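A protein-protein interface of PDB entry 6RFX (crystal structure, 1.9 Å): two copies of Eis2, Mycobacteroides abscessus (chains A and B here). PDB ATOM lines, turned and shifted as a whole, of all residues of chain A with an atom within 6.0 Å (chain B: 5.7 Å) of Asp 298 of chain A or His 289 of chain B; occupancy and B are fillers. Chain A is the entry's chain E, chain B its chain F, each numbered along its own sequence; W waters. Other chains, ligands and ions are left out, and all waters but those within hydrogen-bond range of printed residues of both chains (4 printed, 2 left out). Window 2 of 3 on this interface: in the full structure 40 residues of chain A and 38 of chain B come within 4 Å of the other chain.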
ATOM      1  N   ALA A 118      13.464  28.575   9.474  1.00  0.00           N
ATOM      2  CA  ALA A 118      12.246  28.796  10.245  1.00  0.00           C
ATOM      3  C   ALA A 118      11.406  29.938   9.694  1.00  0.00           C
ATOM      4  O   ALA A 118      10.224  30.043  10.035  1.00  0.00           O
ATOM      5  CB  ALA A 118      12.585  29.056  11.713  1.00  0.00           C
ATOM      6  N   TYR A 124       6.021  25.664   9.649  1.00  0.00           N
ATOM      7  CA  TYR A 124       6.769  25.792  10.892  1.00  0.00           C
ATOM      8  C   TYR A 124       6.214  24.843  11.947  1.00  0.00           C
ATOM      9  O   TYR A 124       5.034  24.916  12.302  1.00  0.00           O
ATOM     10  CB  TYR A 124       6.696  27.234  11.393  1.00  0.00           C
ATOM     11  CG  TYR A 124       7.391  27.442  12.719  1.00  0.00           C
ATOM     12  CD1 TYR A 124       8.742  27.760  12.773  1.00  0.00           C
ATOM     13  CD2 TYR A 124       6.700  27.312  13.917  1.00  0.00           C
ATOM     14  CE1 TYR A 124       9.384  27.947  13.984  1.00  0.00           C
ATOM     15  CE2 TYR A 124       7.333  27.494  15.131  1.00  0.00           C
ATOM     16  CZ  TYR A 124       8.674  27.811  15.159  1.00  0.00           C
ATOM     17  OH  TYR A 124       9.304  27.992  16.367  1.00  0.00           O
ATOM     18  N   VAL A 131      12.819  22.465  15.207  1.00  0.00           N
ATOM     19  CA  VAL A 131      13.878  23.469  15.250  1.00  0.00           C
ATOM     20  C   VAL A 131      15.105  22.863  15.911  1.00  0.00           C
ATOM     21  O   VAL A 131      15.062  22.450  17.077  1.00  0.00           O
ATOM     22  CB  VAL A 131      13.400  24.730  15.976  1.00  0.00           C
ATOM     23  CG1 VAL A 131      14.575  25.661  16.245  1.00  0.00           C
ATOM     24  CG2 VAL A 131      12.337  25.447  15.150  1.00  0.00           C
ATOM     25  N   THR A 133      18.548  24.294  15.170  1.00  0.00           N
ATOM     26  CA  THR A 133      19.651  25.238  15.176  1.00  0.00           C
ATOM     27  C   THR A 133      19.092  26.631  15.413  1.00  0.00           C
ATOM     28  O   THR A 133      18.027  26.976  14.895  1.00  0.00           O
ATOM     29  CB  THR A 133      20.400  25.198  13.836  1.00  0.00           C
ATOM     30  OG1 THR A 133      21.020  23.915  13.674  1.00  0.00           O
ATOM     31  CG2 THR A 133      21.468  26.277  13.774  1.00  0.00           C
ATOM     32  N   GLU A 134      19.805  27.420  16.206  1.00  0.00           N
ATOM     33  CA  GLU A 134      19.433  28.798  16.467  1.00  0.00           C
ATOM     34  C   GLU A 134      20.468  29.740  15.868  1.00  0.00           C
ATOM     35  O   GLU A 134      21.591  29.344  15.539  1.00  0.00           O
ATOM     36  CB  GLU A 134      19.310  29.054  17.973  1.00  0.00           C
ATOM     37  CG  GLU A 134      18.311  28.153  18.674  1.00  0.00           C
ATOM     38  CD  GLU A 134      18.219  28.439  20.159  1.00  0.00           C
ATOM     39  OE1 GLU A 134      17.143  28.875  20.620  1.00  0.00           O
ATOM     40  OE2 GLU A 134      19.230  28.238  20.863  1.00  0.00           O
ATOM     41  N   SER A 135      20.067  30.997  15.712  1.00  0.00           N
ATOM     42  CA  SER A 135      20.974  32.059  15.309  1.00  0.00           C
ATOM     43  C   SER A 135      20.816  33.231  16.265  1.00  0.00           C
ATOM     44  O   SER A 135      19.766  33.410  16.891  1.00  0.00           O
ATOM     45  CB  SER A 135      20.727  32.516  13.863  1.00  0.00           C
ATOM     46  OG  SER A 135      19.431  33.067  13.713  1.00  0.00           O
ATOM     47  N   VAL A 296      18.411  35.637  20.505  1.00  0.00           N
ATOM     48  CA  VAL A 296      18.454  34.281  19.965  1.00  0.00           C
ATOM     49  C   VAL A 296      17.100  33.939  19.361  1.00  0.00           C
ATOM     50  O   VAL A 296      16.052  34.216  19.960  1.00  0.00           O
ATOM     51  CB  VAL A 296      18.845  33.275  21.063  1.00  0.00           C
ATOM     52  CG1 VAL A 296      18.811  31.852  20.529  1.00  0.00           C
ATOM     53  CG2 VAL A 296      20.219  33.605  21.619  1.00  0.00           C
ATOM     54  N   SER A 297      17.116  33.332  18.174  1.00  0.00           N
ATOM     55  CA  SER A 297      15.889  32.939  17.495  1.00  0.00           C
ATOM     56  C   SER A 297      16.138  31.661  16.704  1.00  0.00           C
ATOM     57  O   SER A 297      17.279  31.218  16.540  1.00  0.00           O
ATOM     58  CB  SER A 297      15.367  34.053  16.582  1.00  0.00           C
ATOM     59  OG  SER A 297      16.293  34.339  15.550  1.00  0.00           O
ATOM     60  N   ASP A 298      15.049  31.070  16.215  1.00  0.00           N
ATOM     61  CA  ASP A 298      15.147  29.858  15.415  1.00  0.00           C
ATOM     62  C   ASP A 298      15.905  30.128  14.124  1.00  0.00           C
ATOM     63  O   ASP A 298      15.844  31.224  13.555  1.00  0.00           O
ATOM     64  CB  ASP A 298      13.756  29.355  15.037  1.00  0.00           C
ATOM     65  CG  ASP A 298      12.925  28.970  16.230  1.00  0.00           C
ATOM     66  OD1 ASP A 298      13.500  28.640  17.288  1.00  0.00           O
ATOM     67  OD2 ASP A 298      11.685  28.988  16.092  1.00  0.00           O
ATOM     68  N   ALA A 299      16.610  29.102  13.648  1.00  0.00           N
ATOM     69  CA  ALA A 299      17.302  29.173  12.364  1.00  0.00           C
ATOM     70  C   ALA A 299      16.886  28.023  11.455  1.00  0.00           C
ATOM     71  O   ALA A 299      16.119  28.244  10.515  1.00  0.00           O
ATOM     72  CB  ALA A 299      18.819  29.232  12.559  1.00  0.00           C
ATOM     73  N   ILE A 300      17.347  26.801  11.713  1.00  0.00           N
ATOM     74  CA  ILE A 300      17.152  25.667  10.819  1.00  0.00           C
ATOM     75  C   ILE A 300      16.250  24.644  11.496  1.00  0.00           C
ATOM     76  O   ILE A 300      16.459  24.298  12.665  1.00  0.00           O
ATOM     77  CB  ILE A 300      18.498  25.035  10.426  1.00  0.00           C
ATOM     78  CG1 ILE A 300      19.283  25.980   9.515  1.00  0.00           C
ATOM     79  CG2 ILE A 300      18.291  23.677   9.766  1.00  0.00           C
ATOM     80  CD1 ILE A 300      18.559  26.327   8.232  1.00  0.00           C
ATOM     81  N   ARG A 363       9.973  14.699  15.552  1.00  0.00           N
ATOM     82  CA  ARG A 363      10.211  16.137  15.573  1.00  0.00           C
ATOM     83  C   ARG A 363      11.260  16.501  16.617  1.00  0.00           C
ATOM     84  O   ARG A 363      12.195  17.261  16.339  1.00  0.00           O
ATOM     85  CB  ARG A 363       8.902  16.872  15.852  1.00  0.00           C
ATOM     86  CG  ARG A 363       9.084  18.334  16.217  1.00  0.00           C
ATOM     87  CD  ARG A 363       7.763  18.987  16.581  1.00  0.00           C
ATOM     88  NE  ARG A 363       7.946  20.378  16.978  1.00  0.00           N
ATOM     89  CZ  ARG A 363       6.953  21.242  17.148  1.00  0.00           C
ATOM     90  NH1 ARG A 363       5.699  20.859  16.951  1.00  0.00           N
ATOM     91  NH2 ARG A 363       7.214  22.492  17.511  1.00  0.00           N
ATOM     92  N   ARG B 283      10.482  28.032  26.868  1.00  0.00           N
ATOM     93  CA  ARG B 283      10.901  28.302  25.494  1.00  0.00           C
ATOM     94  C   ARG B 283      10.546  27.157  24.558  1.00  0.00           C
ATOM     95  O   ARG B 283      10.278  27.383  23.371  1.00  0.00           O
ATOM     96  CB  ARG B 283      12.406  28.560  25.439  1.00  0.00           C
ATOM     97  CG  ARG B 283      12.879  29.760  26.242  1.00  0.00           C
ATOM     98  CD  ARG B 283      14.331  30.055  25.922  1.00  0.00           C
ATOM     99  NE  ARG B 283      14.500  30.397  24.515  1.00  0.00           N
ATOM    100  CZ  ARG B 283      15.609  30.175  23.816  1.00  0.00           C
ATOM    101  NH1 ARG B 283      16.656  29.599  24.392  1.00  0.00           N
ATOM    102  NH2 ARG B 283      15.666  30.523  22.537  1.00  0.00           N
ATOM    103  N   TYR B 284      10.539  25.927  25.067  1.00  0.00           N
ATOM    104  CA  TYR B 284      10.243  24.756  24.257  1.00  0.00           C
ATOM    105  C   TYR B 284       8.790  24.317  24.356  1.00  0.00           C
ATOM    106  O   TYR B 284       8.344  23.516  23.528  1.00  0.00           O
ATOM    107  CB  TYR B 284      11.193  23.610  24.630  1.00  0.00           C
ATOM    108  CG  TYR B 284      12.637  24.060  24.625  1.00  0.00           C
ATOM    109  CD1 TYR B 284      13.366  24.104  23.442  1.00  0.00           C
ATOM    110  CD2 TYR B 284      13.261  24.475  25.793  1.00  0.00           C
ATOM    111  CE1 TYR B 284      14.679  24.530  23.427  1.00  0.00           C
ATOM    112  CE2 TYR B 284      14.574  24.903  25.789  1.00  0.00           C
ATOM    113  CZ  TYR B 284      15.277  24.930  24.602  1.00  0.00           C
ATOM    114  OH  TYR B 284      16.586  25.357  24.589  1.00  0.00           O
ATOM    115  N   LEU B 285       8.044  24.829  25.338  1.00  0.00           N
ATOM    116  CA  LEU B 285       6.610  24.574  25.398  1.00  0.00           C
ATOM    117  C   LEU B 285       5.846  25.398  24.371  1.00  0.00           C
ATOM    118  O   LEU B 285       4.854  24.918  23.812  1.00  0.00           O
ATOM    119  CB  LEU B 285       6.083  24.872  26.804  1.00  0.00           C
ATOM    120  CG  LEU B 285       6.696  24.040  27.933  1.00  0.00           C
ATOM    121  CD1 LEU B 285       6.072  24.401  29.272  1.00  0.00           C
ATOM    122  CD2 LEU B 285       6.544  22.551  27.642  1.00  0.00           C
ATOM    123  N   VAL B 286       6.299  26.626  24.105  1.00  0.00           N
ATOM    124  CA  VAL B 286       5.610  27.513  23.175  1.00  0.00           C
ATOM    125  C   VAL B 286       5.650  26.924  21.770  1.00  0.00           C
ATOM    126  O   VAL B 286       6.692  26.443  21.304  1.00  0.00           O
ATOM    127  CB  VAL B 286       6.250  28.912  23.218  1.00  0.00           C
ATOM    128  CG1 VAL B 286       5.583  29.843  22.217  1.00  0.00           C
ATOM    129  CG2 VAL B 286       6.159  29.488  24.622  1.00  0.00           C
ATOM    130  N   ALA B 287       4.503  26.957  21.086  1.00  0.00           N
ATOM    131  CA  ALA B 287       4.418  26.369  19.752  1.00  0.00           C
ATOM    132  C   ALA B 287       5.171  27.205  18.726  1.00  0.00           C
ATOM    133  O   ALA B 287       5.847  26.657  17.847  1.00  0.00           O
ATOM    134  CB  ALA B 287       2.956  26.199  19.343  1.00  0.00           C
ATOM    135  N   ASN B 288       5.069  28.526  18.816  1.00  0.00           N
ATOM    136  CA  ASN B 288       5.717  29.438  17.879  1.00  0.00           C
ATOM    137  C   ASN B 288       6.842  30.147  18.627  1.00  0.00           C
ATOM    138  O   ASN B 288       6.609  31.158  19.297  1.00  0.00           O
ATOM    139  CB  ASN B 288       4.703  30.439  17.332  1.00  0.00           C
ATOM    140  CG  ASN B 288       5.252  31.252  16.173  1.00  0.00           C
ATOM    141  OD1 ASN B 288       5.807  30.702  15.223  1.00  0.00           O
ATOM    142  ND2 ASN B 288       5.103  32.571  16.250  1.00  0.00           N
ATOM    143  N   HIS B 289       8.058  29.612  18.513  1.00  0.00           N
ATOM    144  CA  HIS B 289       9.214  30.225  19.167  1.00  0.00           C
ATOM    145  C   HIS B 289       9.409  31.704  18.841  1.00  0.00           C
ATOM    146  O   HIS B 289       9.737  32.466  19.767  1.00  0.00           O
ATOM    147  CB  HIS B 289      10.504  29.442  18.876  1.00  0.00           C
ATOM    148  CG  HIS B 289      10.511  28.041  19.402  1.00  0.00           C
ATOM    149  ND1 HIS B 289      11.544  27.163  19.153  1.00  0.00           N
ATOM    150  CD2 HIS B 289       9.619  27.366  20.165  1.00  0.00           C
ATOM    151  CE1 HIS B 289      11.288  26.006  19.739  1.00  0.00           C
ATOM    152  NE2 HIS B 289      10.126  26.103  20.358  1.00  0.00           N
ATOM    153  N   PRO B 290       9.261  32.173  17.595  1.00  0.00           N
ATOM    154  CA  PRO B 290       9.441  33.613  17.333  1.00  0.00           C
ATOM    155  C   PRO B 290       8.548  34.520  18.166  1.00  0.00           C
ATOM    156  O   PRO B 290       8.869  35.705  18.317  1.00  0.00           O
ATOM    157  CB  PRO B 290       9.137  33.744  15.835  1.00  0.00           C
ATOM    158  CG  PRO B 290       9.481  32.415  15.277  1.00  0.00           C
ATOM    159  CD  PRO B 290       9.110  31.415  16.335  1.00  0.00           C
ATOM    160  N   SER B 291       7.442  34.009  18.713  1.00  0.00           N
ATOM    161  CA  SER B 291       6.568  34.835  19.536  1.00  0.00           C
ATOM    162  C   SER B 291       7.166  35.132  20.906  1.00  0.00           C
ATOM    163  O   SER B 291       6.755  36.104  21.548  1.00  0.00           O
ATOM    164  CB  SER B 291       5.196  34.173  19.689  1.00  0.00           C
ATOM    165  OG  SER B 291       4.553  34.026  18.436  1.00  0.00           O
ATOM    166  N   LEU B 292       8.117  34.326  21.369  1.00  0.00           N
ATOM    167  CA  LEU B 292       8.764  34.526  22.664  1.00  0.00           C
ATOM    168  C   LEU B 292      10.193  34.992  22.403  1.00  0.00           C
ATOM    169  O   LEU B 292      11.085  34.178  22.147  1.00  0.00           O
ATOM    170  CB  LEU B 292       8.740  33.243  23.493  1.00  0.00           C
ATOM    171  CG  LEU B 292       9.244  33.365  24.934  1.00  0.00           C
ATOM    172  CD1 LEU B 292       8.304  34.225  25.770  1.00  0.00           C
ATOM    173  CD2 LEU B 292       9.427  31.994  25.568  1.00  0.00           C
ATOM    174  N   GLU B 293      10.402  36.306  22.464  1.00  0.00           N
ATOM    175  CA  GLU B 293      11.731  36.865  22.267  1.00  0.00           C
ATOM    176  C   GLU B 293      12.651  36.448  23.404  1.00  0.00           C
ATOM    177  O   GLU B 293      12.251  36.420  24.572  1.00  0.00           O
ATOM    178  CB  GLU B 293      11.653  38.390  22.209  1.00  0.00           C
ATOM    179  CG  GLU B 293      13.003  39.068  22.028  1.00  0.00           C
ATOM    180  CD  GLU B 293      12.915  40.582  22.086  1.00  0.00           C
ATOM    181  OE1 GLU B 293      12.406  41.117  23.096  1.00  0.00           O
ATOM    182  OE2 GLU B 293      13.354  41.238  21.117  1.00  0.00           O
HETATM  183  O   HOH W   1      17.868  25.926  22.205  1.00  0.00           O
HETATM  184  O   HOH W   2       5.154  24.111  16.981  1.00  0.00           O
HETATM  185  O   HOH W   3      19.172  28.943  23.299  1.00  0.00           O
HETATM  186  O   HOH W   4       7.651  24.487  19.131  1.00  0.00           O
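Val 131 of chain A touches none of the printed residues of chain B. Of the printed residues of chain B, Val 296 of chain A touches Arg 283. Asp 298 of chain A touches two residues of chain B. Of the printed residues of chain A, Ala 287 of chain B touches Tyr 124. Of chain A, only Tyr 124 and Asp 298 come within 4 Å of His 289 of chain B. The nearest printed residue of chain A that does not touch Ala 287 of chain B is Arg 363 of chain A (4.4 Å).
Among the printed residues, merely in contact across the chains: Tyr 124 of chain A with Ala 287 of chain B, Tyr 124 of chain A with Asn 288 of chain B, Tyr 124 of chain A with Pro 290 of chain B, Val 296 of chain A with Arg 283 of chain B and Asp 298 of chain A with Pro 290 of chain B.
No position is printed for both chains.
Water W3 lies within hydrogen-bond range of OE2 of Glu 134 of chain A (2.5 Å) and NH1 of Arg 283 of chain B (2.8 Å). Water W4 lies within hydrogen-bond range of the guanidinium group of Arg 363 of chain A (2.6 Å), the backbone carbonyl oxygen of Val 286 of chain B (3.1 Å), the backbone carbonyl oxygen of Ala 287 of chain B (3.1 Å) and a ring nitrogen (NE2) of His 289 of chain B (3.2 Å). Water W2 bridges NH2 of Arg 363 of chain A (2.7 Å) and O of Ala 287 of chain B (2.8 Å). Water W1 bridges OH of Tyr 284 of chain B and OE2 of Glu 134 of chain A.
Of the 11 printed residues of chain B, 5 touch a printed residue of chain A. Hydrophobic or aromatic side chains of chain B within 4 Å of the printed part of chain A: His 289 and Pro 290. Hydrophobic or aromatic side chains of chain A within 4 Å of the printed part of chain B: Tyr 124 and Val 296.
OD2 of Asp 298 of chain A is in hydrogen-bond range of OH of Tyr 124 of chain A (2.6 Å). The backbone carbonyl oxygen of Arg 283 of chain B lies close to a ring nitrogen (NE2) of His 289 of chain B (3.3 Å). The side-chain amide nitrogen (ND2) of Asn 288 of chain B sits at hydrogen-bond distance from the side-chain hydroxyl (OG) of Ser 291 of chain B (2.7 Å).
A ring nitrogen (ND1) of His 289 of chain B sits at hydrogen-bond distance from the side-chain carboxylate of Asp 298 of chain A, at 3.1 Å. The side-chain carboxylate (OE1) of Glu 134 of chain A is in salt-bridge range of the guanidinium group (NH2) of Arg 283 of chain B (2.9 Å). OH of Tyr 124 of chain A is in hydrogen-bond range of N of His 289 of chain B, at 3.0 Å.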
